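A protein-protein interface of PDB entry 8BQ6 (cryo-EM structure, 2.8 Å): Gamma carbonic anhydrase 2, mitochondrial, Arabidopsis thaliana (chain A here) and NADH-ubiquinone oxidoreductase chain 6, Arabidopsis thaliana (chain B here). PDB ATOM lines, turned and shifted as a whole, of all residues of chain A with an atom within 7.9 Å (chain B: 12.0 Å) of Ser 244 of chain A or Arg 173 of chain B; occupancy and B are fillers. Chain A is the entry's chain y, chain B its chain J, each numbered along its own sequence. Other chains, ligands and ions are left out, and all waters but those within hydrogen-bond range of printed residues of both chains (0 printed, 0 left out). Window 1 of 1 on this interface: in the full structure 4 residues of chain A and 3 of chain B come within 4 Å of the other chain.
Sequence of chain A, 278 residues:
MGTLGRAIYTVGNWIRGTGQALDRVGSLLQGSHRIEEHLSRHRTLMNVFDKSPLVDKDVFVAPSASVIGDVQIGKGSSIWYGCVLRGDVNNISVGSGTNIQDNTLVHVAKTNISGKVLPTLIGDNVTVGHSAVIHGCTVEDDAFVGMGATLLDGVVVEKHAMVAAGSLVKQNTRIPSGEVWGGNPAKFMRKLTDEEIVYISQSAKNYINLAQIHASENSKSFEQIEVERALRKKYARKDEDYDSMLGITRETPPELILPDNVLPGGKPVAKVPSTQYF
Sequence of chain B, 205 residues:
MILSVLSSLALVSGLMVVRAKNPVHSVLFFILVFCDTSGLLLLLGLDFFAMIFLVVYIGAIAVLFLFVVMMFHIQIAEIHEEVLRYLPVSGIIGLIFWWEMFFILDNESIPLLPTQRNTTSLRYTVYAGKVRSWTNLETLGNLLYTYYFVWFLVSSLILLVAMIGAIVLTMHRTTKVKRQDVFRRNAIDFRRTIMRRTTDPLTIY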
ATOM      1  N   ASP A 239     -34.700  -6.232   5.087  1.00  0.00           N
ATOM      2  CA  ASP A 239     -34.542  -6.034   6.528  1.00  0.00           C
ATOM      3  C   ASP A 239     -34.225  -4.560   6.731  1.00  0.00           C
ATOM      4  O   ASP A 239     -33.060  -4.168   6.801  1.00  0.00           O
ATOM      5  CB  ASP A 239     -33.460  -6.918   7.099  1.00  0.00           C
ATOM      6  CG  ASP A 239     -33.491  -6.977   8.615  1.00  0.00           C
ATOM      7  OD1 ASP A 239     -34.311  -6.267   9.229  1.00  0.00           O
ATOM      8  OD2 ASP A 239     -32.713  -7.759   9.195  1.00  0.00           O
ATOM      9  N   GLU A 240     -35.269  -3.739   6.829  1.00  0.00           N
ATOM     10  CA  GLU A 240     -35.042  -2.314   7.023  1.00  0.00           C
ATOM     11  C   GLU A 240     -34.606  -2.003   8.446  1.00  0.00           C
ATOM     12  O   GLU A 240     -33.977  -0.967   8.688  1.00  0.00           O
ATOM     13  CB  GLU A 240     -36.294  -1.532   6.642  1.00  0.00           C
ATOM     14  CG  GLU A 240     -36.806  -1.932   5.284  1.00  0.00           C
ATOM     15  CD  GLU A 240     -37.423  -0.784   4.514  1.00  0.00           C
ATOM     16  OE1 GLU A 240     -36.781  -0.323   3.546  1.00  0.00           O
ATOM     17  OE2 GLU A 240     -38.552  -0.366   4.842  1.00  0.00           O
ATOM     18  N   ASP A 241     -34.900  -2.892   9.390  1.00  0.00           N
ATOM     19  CA  ASP A 241     -34.406  -2.702  10.747  1.00  0.00           C
ATOM     20  C   ASP A 241     -32.888  -2.830  10.812  1.00  0.00           C
ATOM     21  O   ASP A 241     -32.202  -1.953  11.359  1.00  0.00           O
ATOM     22  CB  ASP A 241     -35.063  -3.714  11.670  1.00  0.00           C
ATOM     23  CG  ASP A 241     -34.963  -3.316  13.103  1.00  0.00           C
ATOM     24  OD1 ASP A 241     -34.671  -2.133  13.371  1.00  0.00           O
ATOM     25  OD2 ASP A 241     -35.174  -4.186  13.961  1.00  0.00           O
ATOM     26  N   TYR A 242     -32.344  -3.914  10.257  1.00  0.00           N
ATOM     27  CA  TYR A 242     -30.897  -4.075  10.245  1.00  0.00           C
ATOM     28  C   TYR A 242     -30.228  -3.014   9.389  1.00  0.00           C
ATOM     29  O   TYR A 242     -29.114  -2.577   9.700  1.00  0.00           O
ATOM     30  CB  TYR A 242     -30.517  -5.468   9.752  1.00  0.00           C
ATOM     31  CG  TYR A 242     -29.133  -5.863  10.177  1.00  0.00           C
ATOM     32  CD1 TYR A 242     -28.866  -6.195  11.492  1.00  0.00           C
ATOM     33  CD2 TYR A 242     -28.089  -5.885   9.270  1.00  0.00           C
ATOM     34  CE1 TYR A 242     -27.608  -6.543  11.890  1.00  0.00           C
ATOM     35  CE2 TYR A 242     -26.823  -6.236   9.661  1.00  0.00           C
ATOM     36  CZ  TYR A 242     -26.587  -6.565  10.975  1.00  0.00           C
ATOM     37  OH  TYR A 242     -25.325  -6.920  11.384  1.00  0.00           O
ATOM     38  N   ASP A 243     -30.891  -2.592   8.312  1.00  0.00           N
ATOM     39  CA  ASP A 243     -30.374  -1.493   7.507  1.00  0.00           C
ATOM     40  C   ASP A 243     -30.284  -0.205   8.311  1.00  0.00           C
ATOM     41  O   ASP A 243     -29.311   0.546   8.182  1.00  0.00           O
ATOM     42  CB  ASP A 243     -31.254  -1.279   6.281  1.00  0.00           C
ATOM     43  CG  ASP A 243     -30.925  -2.232   5.166  1.00  0.00           C
ATOM     44  OD1 ASP A 243     -31.863  -2.731   4.515  1.00  0.00           O
ATOM     45  OD2 ASP A 243     -29.726  -2.480   4.938  1.00  0.00           O
ATOM     46  N   SER A 244     -31.302   0.088   9.124  1.00  0.00           N
ATOM     47  CA  SER A 244     -31.238   1.297   9.935  1.00  0.00           C
ATOM     48  C   SER A 244     -30.159   1.175  11.000  1.00  0.00           C
ATOM     49  O   SER A 244     -29.537   2.174  11.379  1.00  0.00           O
ATOM     50  CB  SER A 244     -32.596   1.594  10.569  1.00  0.00           C
ATOM     51  OG  SER A 244     -32.697   1.018  11.857  1.00  0.00           O
ATOM     52  N   MET A 245     -29.917  -0.044  11.492  1.00  0.00           N
ATOM     53  CA  MET A 245     -28.790  -0.242  12.402  1.00  0.00           C
ATOM     54  C   MET A 245     -27.465   0.051  11.709  1.00  0.00           C
ATOM     55  O   MET A 245     -26.586   0.704  12.284  1.00  0.00           O
ATOM     56  CB  MET A 245     -28.786  -1.660  12.966  1.00  0.00           C
ATOM     57  CG  MET A 245     -27.743  -1.855  14.060  1.00  0.00           C
ATOM     58  SD  MET A 245     -27.124  -3.537  14.190  1.00  0.00           S
ATOM     59  CE  MET A 245     -26.003  -3.547  12.800  1.00  0.00           C
ATOM     60  N   LEU A 246     -27.297  -0.435  10.477  1.00  0.00           N
ATOM     61  CA  LEU A 246     -26.113  -0.120   9.687  1.00  0.00           C
ATOM     62  C   LEU A 246     -26.096   1.320   9.198  1.00  0.00           C
ATOM     63  O   LEU A 246     -25.036   1.803   8.785  1.00  0.00           O
ATOM     64  CB  LEU A 246     -26.019  -1.050   8.481  1.00  0.00           C
ATOM     65  CG  LEU A 246     -25.599  -2.493   8.741  1.00  0.00           C
ATOM     66  CD1 LEU A 246     -26.031  -3.378   7.586  1.00  0.00           C
ATOM     67  CD2 LEU A 246     -24.103  -2.568   8.943  1.00  0.00           C
ATOM     68  N   GLY A 247     -27.231   2.008   9.234  1.00  0.00           N
ATOM     69  CA  GLY A 247     -27.334   3.343   8.675  1.00  0.00           C
ATOM     70  C   GLY A 247     -27.207   3.404   7.169  1.00  0.00           C
ATOM     71  O   GLY A 247     -26.530   4.295   6.644  1.00  0.00           O
ATOM     72  N   ILE A 248     -27.840   2.475   6.455  1.00  0.00           N
ATOM     73  CA  ILE A 248     -27.819   2.472   5.000  1.00  0.00           C
ATOM     74  C   ILE A 248     -29.250   2.363   4.500  1.00  0.00           C
ATOM     75  O   ILE A 248     -30.164   1.986   5.232  1.00  0.00           O
ATOM     76  CB  ILE A 248     -26.960   1.333   4.419  1.00  0.00           C
ATOM     77  CG1 ILE A 248     -27.606  -0.013   4.719  1.00  0.00           C
ATOM     78  CG2 ILE A 248     -25.562   1.376   4.983  1.00  0.00           C
ATOM     79  CD1 ILE A 248     -27.044  -1.124   3.918  1.00  0.00           C
ATOM     80  N   THR A 249     -29.439   2.718   3.234  1.00  0.00           N
ATOM     81  CA  THR A 249     -30.752   2.682   2.602  1.00  0.00           C
ATOM     82  C   THR A 249     -30.610   1.963   1.273  1.00  0.00           C
ATOM     83  O   THR A 249     -30.079   2.527   0.313  1.00  0.00           O
ATOM     84  CB  THR A 249     -31.316   4.087   2.404  1.00  0.00           C
ATOM     85  OG1 THR A 249     -31.155   4.838   3.611  1.00  0.00           O
ATOM     86  CG2 THR A 249     -32.794   4.024   2.037  1.00  0.00           C
ATOM     87  N   ALA B 166     -26.223  -4.469  23.843  1.00  0.00           N
ATOM     88  CA  ALA B 166     -26.511  -3.040  23.836  1.00  0.00           C
ATOM     89  C   ALA B 166     -26.432  -2.478  22.427  1.00  0.00           C
ATOM     90  O   ALA B 166     -27.326  -1.738  22.001  1.00  0.00           O
ATOM     91  CB  ALA B 166     -25.551  -2.293  24.758  1.00  0.00           C
ATOM     92  N   ILE B 167     -25.376  -2.820  21.681  1.00  0.00           N
ATOM     93  CA  ILE B 167     -25.272  -2.300  20.319  1.00  0.00           C
ATOM     94  C   ILE B 167     -26.425  -2.807  19.461  1.00  0.00           C
ATOM     95  O   ILE B 167     -27.106  -2.031  18.782  1.00  0.00           O
ATOM     96  CB  ILE B 167     -23.919  -2.665  19.686  1.00  0.00           C
ATOM     97  CG1 ILE B 167     -22.761  -1.918  20.352  1.00  0.00           C
ATOM     98  CG2 ILE B 167     -23.958  -2.366  18.206  1.00  0.00           C
ATOM     99  CD1 ILE B 167     -22.978  -0.453  20.527  1.00  0.00           C
ATOM    100  N   VAL B 168     -26.661  -4.118  19.483  1.00  0.00           N
ATOM    101  CA  VAL B 168     -27.628  -4.718  18.572  1.00  0.00           C
ATOM    102  C   VAL B 168     -29.037  -4.228  18.855  1.00  0.00           C
ATOM    103  O   VAL B 168     -29.821  -4.008  17.926  1.00  0.00           O
ATOM    104  CB  VAL B 168     -27.533  -6.251  18.647  1.00  0.00           C
ATOM    105  CG1 VAL B 168     -28.483  -6.879  17.676  1.00  0.00           C
ATOM    106  CG2 VAL B 168     -26.135  -6.688  18.309  1.00  0.00           C
ATOM    107  N   LEU B 169     -29.387  -4.034  20.122  1.00  0.00           N
ATOM    108  CA  LEU B 169     -30.760  -3.671  20.429  1.00  0.00           C
ATOM    109  C   LEU B 169     -31.075  -2.208  20.123  1.00  0.00           C
ATOM    110  O   LEU B 169     -32.190  -1.908  19.686  1.00  0.00           O
ATOM    111  CB  LEU B 169     -31.048  -3.978  21.889  1.00  0.00           C
ATOM    112  CG  LEU B 169     -31.169  -5.480  22.129  1.00  0.00           C
ATOM    113  CD1 LEU B 169     -31.114  -5.764  23.607  1.00  0.00           C
ATOM    114  CD2 LEU B 169     -32.416  -6.058  21.487  1.00  0.00           C
ATOM    115  N   THR B 170     -30.134  -1.283  20.329  1.00  0.00           N
ATOM    116  CA  THR B 170     -30.479   0.134  20.289  1.00  0.00           C
ATOM    117  C   THR B 170     -29.825   0.953  19.183  1.00  0.00           C
ATOM    118  O   THR B 170     -30.295   2.064  18.926  1.00  0.00           O
ATOM    119  CB  THR B 170     -30.142   0.817  21.625  1.00  0.00           C
ATOM    120  OG1 THR B 170     -28.722   0.832  21.812  1.00  0.00           O
ATOM    121  CG2 THR B 170     -30.808   0.100  22.791  1.00  0.00           C
ATOM    122  N   MET B 171     -28.773   0.465  18.534  1.00  0.00           N
ATOM    123  CA  MET B 171     -28.024   1.311  17.609  1.00  0.00           C
ATOM    124  C   MET B 171     -28.856   1.645  16.376  1.00  0.00           C
ATOM    125  O   MET B 171     -29.397   0.754  15.717  1.00  0.00           O
ATOM    126  CB  MET B 171     -26.728   0.618  17.192  1.00  0.00           C
ATOM    127  CG  MET B 171     -25.825   1.344  16.187  1.00  0.00           C
ATOM    128  SD  MET B 171     -24.841   2.741  16.785  1.00  0.00           S
ATOM    129  CE  MET B 171     -26.053   4.037  17.001  1.00  0.00           C
ATOM    130  N   HIS B 172     -28.968   2.937  16.077  1.00  0.00           N
ATOM    131  CA  HIS B 172     -29.479   3.429  14.797  1.00  0.00           C
ATOM    132  C   HIS B 172     -28.415   4.373  14.256  1.00  0.00           C
ATOM    133  O   HIS B 172     -28.341   5.531  14.675  1.00  0.00           O
ATOM    134  CB  HIS B 172     -30.813   4.145  14.946  1.00  0.00           C
ATOM    135  CG  HIS B 172     -31.968   3.233  15.196  1.00  0.00           C
ATOM    136  ND1 HIS B 172     -32.192   2.637  16.417  1.00  0.00           N
ATOM    137  CD2 HIS B 172     -32.981   2.836  14.391  1.00  0.00           C
ATOM    138  CE1 HIS B 172     -33.284   1.898  16.349  1.00  0.00           C
ATOM    139  NE2 HIS B 172     -33.782   2.002  15.131  1.00  0.00           N
ATOM    140  N   ARG B 173     -27.590   3.883  13.340  1.00  0.00           N
ATOM    141  CA  ARG B 173     -26.489   4.687  12.838  1.00  0.00           C
ATOM    142  C   ARG B 173     -27.007   5.777  11.913  1.00  0.00           C
ATOM    143  O   ARG B 173     -27.873   5.535  11.066  1.00  0.00           O
ATOM    144  CB  ARG B 173     -25.480   3.803  12.114  1.00  0.00           C
ATOM    145  CG  ARG B 173     -24.122   4.434  11.944  1.00  0.00           C
ATOM    146  CD  ARG B 173     -23.129   3.454  11.360  1.00  0.00           C
ATOM    147  NE  ARG B 173     -21.771   3.974  11.433  1.00  0.00           N
ATOM    148  CZ  ARG B 173     -20.673   3.235  11.352  1.00  0.00           C
ATOM    149  NH1 ARG B 173     -20.734   1.923  11.190  1.00  0.00           N
ATOM    150  NH2 ARG B 173     -19.487   3.826  11.437  1.00  0.00           N
ATOM    151  N   THR B 174     -26.479   6.980  12.082  1.00  0.00           N
ATOM    152  CA  THR B 174     -26.824   8.103  11.229  1.00  0.00           C
ATOM    153  C   THR B 174     -26.231   7.950   9.833  1.00  0.00           C
ATOM    154  O   THR B 174     -26.867   8.298   8.837  1.00  0.00           O
ATOM    155  CB  THR B 174     -26.334   9.413  11.841  1.00  0.00           C
ATOM    156  OG1 THR B 174     -24.974   9.252  12.264  1.00  0.00           O
ATOM    157  CG2 THR B 174     -27.184   9.778  13.037  1.00  0.00           C
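The backbone NH of Arg 173 of chain B lies close to the backbone carbonyl oxygen of Met 245 of chain A. N of Arg 173 of chain B sits at hydrogen-bond distance from O of Ser 244 of chain A, at 3.2 Å.
The backbone carbonyl oxygen of Asp 241 of chain A is in hydrogen-bond range of the side-chain hydroxyl of Ser 244 of chain A, 3.1 Å away. A ring nitrogen (ND1) of His 172 of chain B lies within hydrogen-bond range of the backbone carbonyl oxygen of Thr 170 of chain B, at 3.2 Å.
Among the printed residues, pairs that only touch across the chains: Ser 244 of chain A with His 172 of chain B, Gly 247 of chain A with Arg 173 of chain B, Met 245 of chain A with Met 171 of chain B and Leu 246 of chain A with Arg 173 of chain B.
No residue of chain B comes within 4 Å of Asp 241 of chain A. Asp 243 of chain A touches none of the printed residues of chain B. Of chain B, only Met 171 and Arg 173 come within 4 Å of Met 245 of chain A. Leu 246 of chain A touches just one residue of chain B: Arg 173 (3.6 Å). Of chain B, only Arg 173 (3.3 Å) comes within 4 Å of Gly 247 of chain A. Val 168 of chain B touches none of the printed residues of chain A. Printed residues of chain A within 4 Å of Met 171 of chain B: Met 245. Of the printed residues of chain A, His 172 of chain B touches Ser 244 (3.1 Å). The nearest residue of chain B that does not touch Ser 244 of chain A is Met 171 of chain B (4.6 Å). The nearest residue of chain A that does not touch Arg 173 of chain B is Ile 248 of chain A (5.5 Å).
Of the 11 printed residues of chain A, 4 touch a printed residue of chain B. Printed residues of chain A that touch a printed residue of chain B: Ser 244, Met 245, Leu 246 and Gly 247. Hydrophobic or aromatic side chains of chain A that line the printed part of chain B: Met 245. Of the 9 printed residues of chain B, 3 touch a printed residue of chain A. Hydrophobic or aromatic side chains of chain B within 4 Å of the printed part of chain A: His 172. Among the printed residues, 6 pairs touch across the chains. Among the printed residues, no Asp or Glu carboxylate lies within 4 Å of a Lys or Arg side-chain nitrogen of the other chain.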
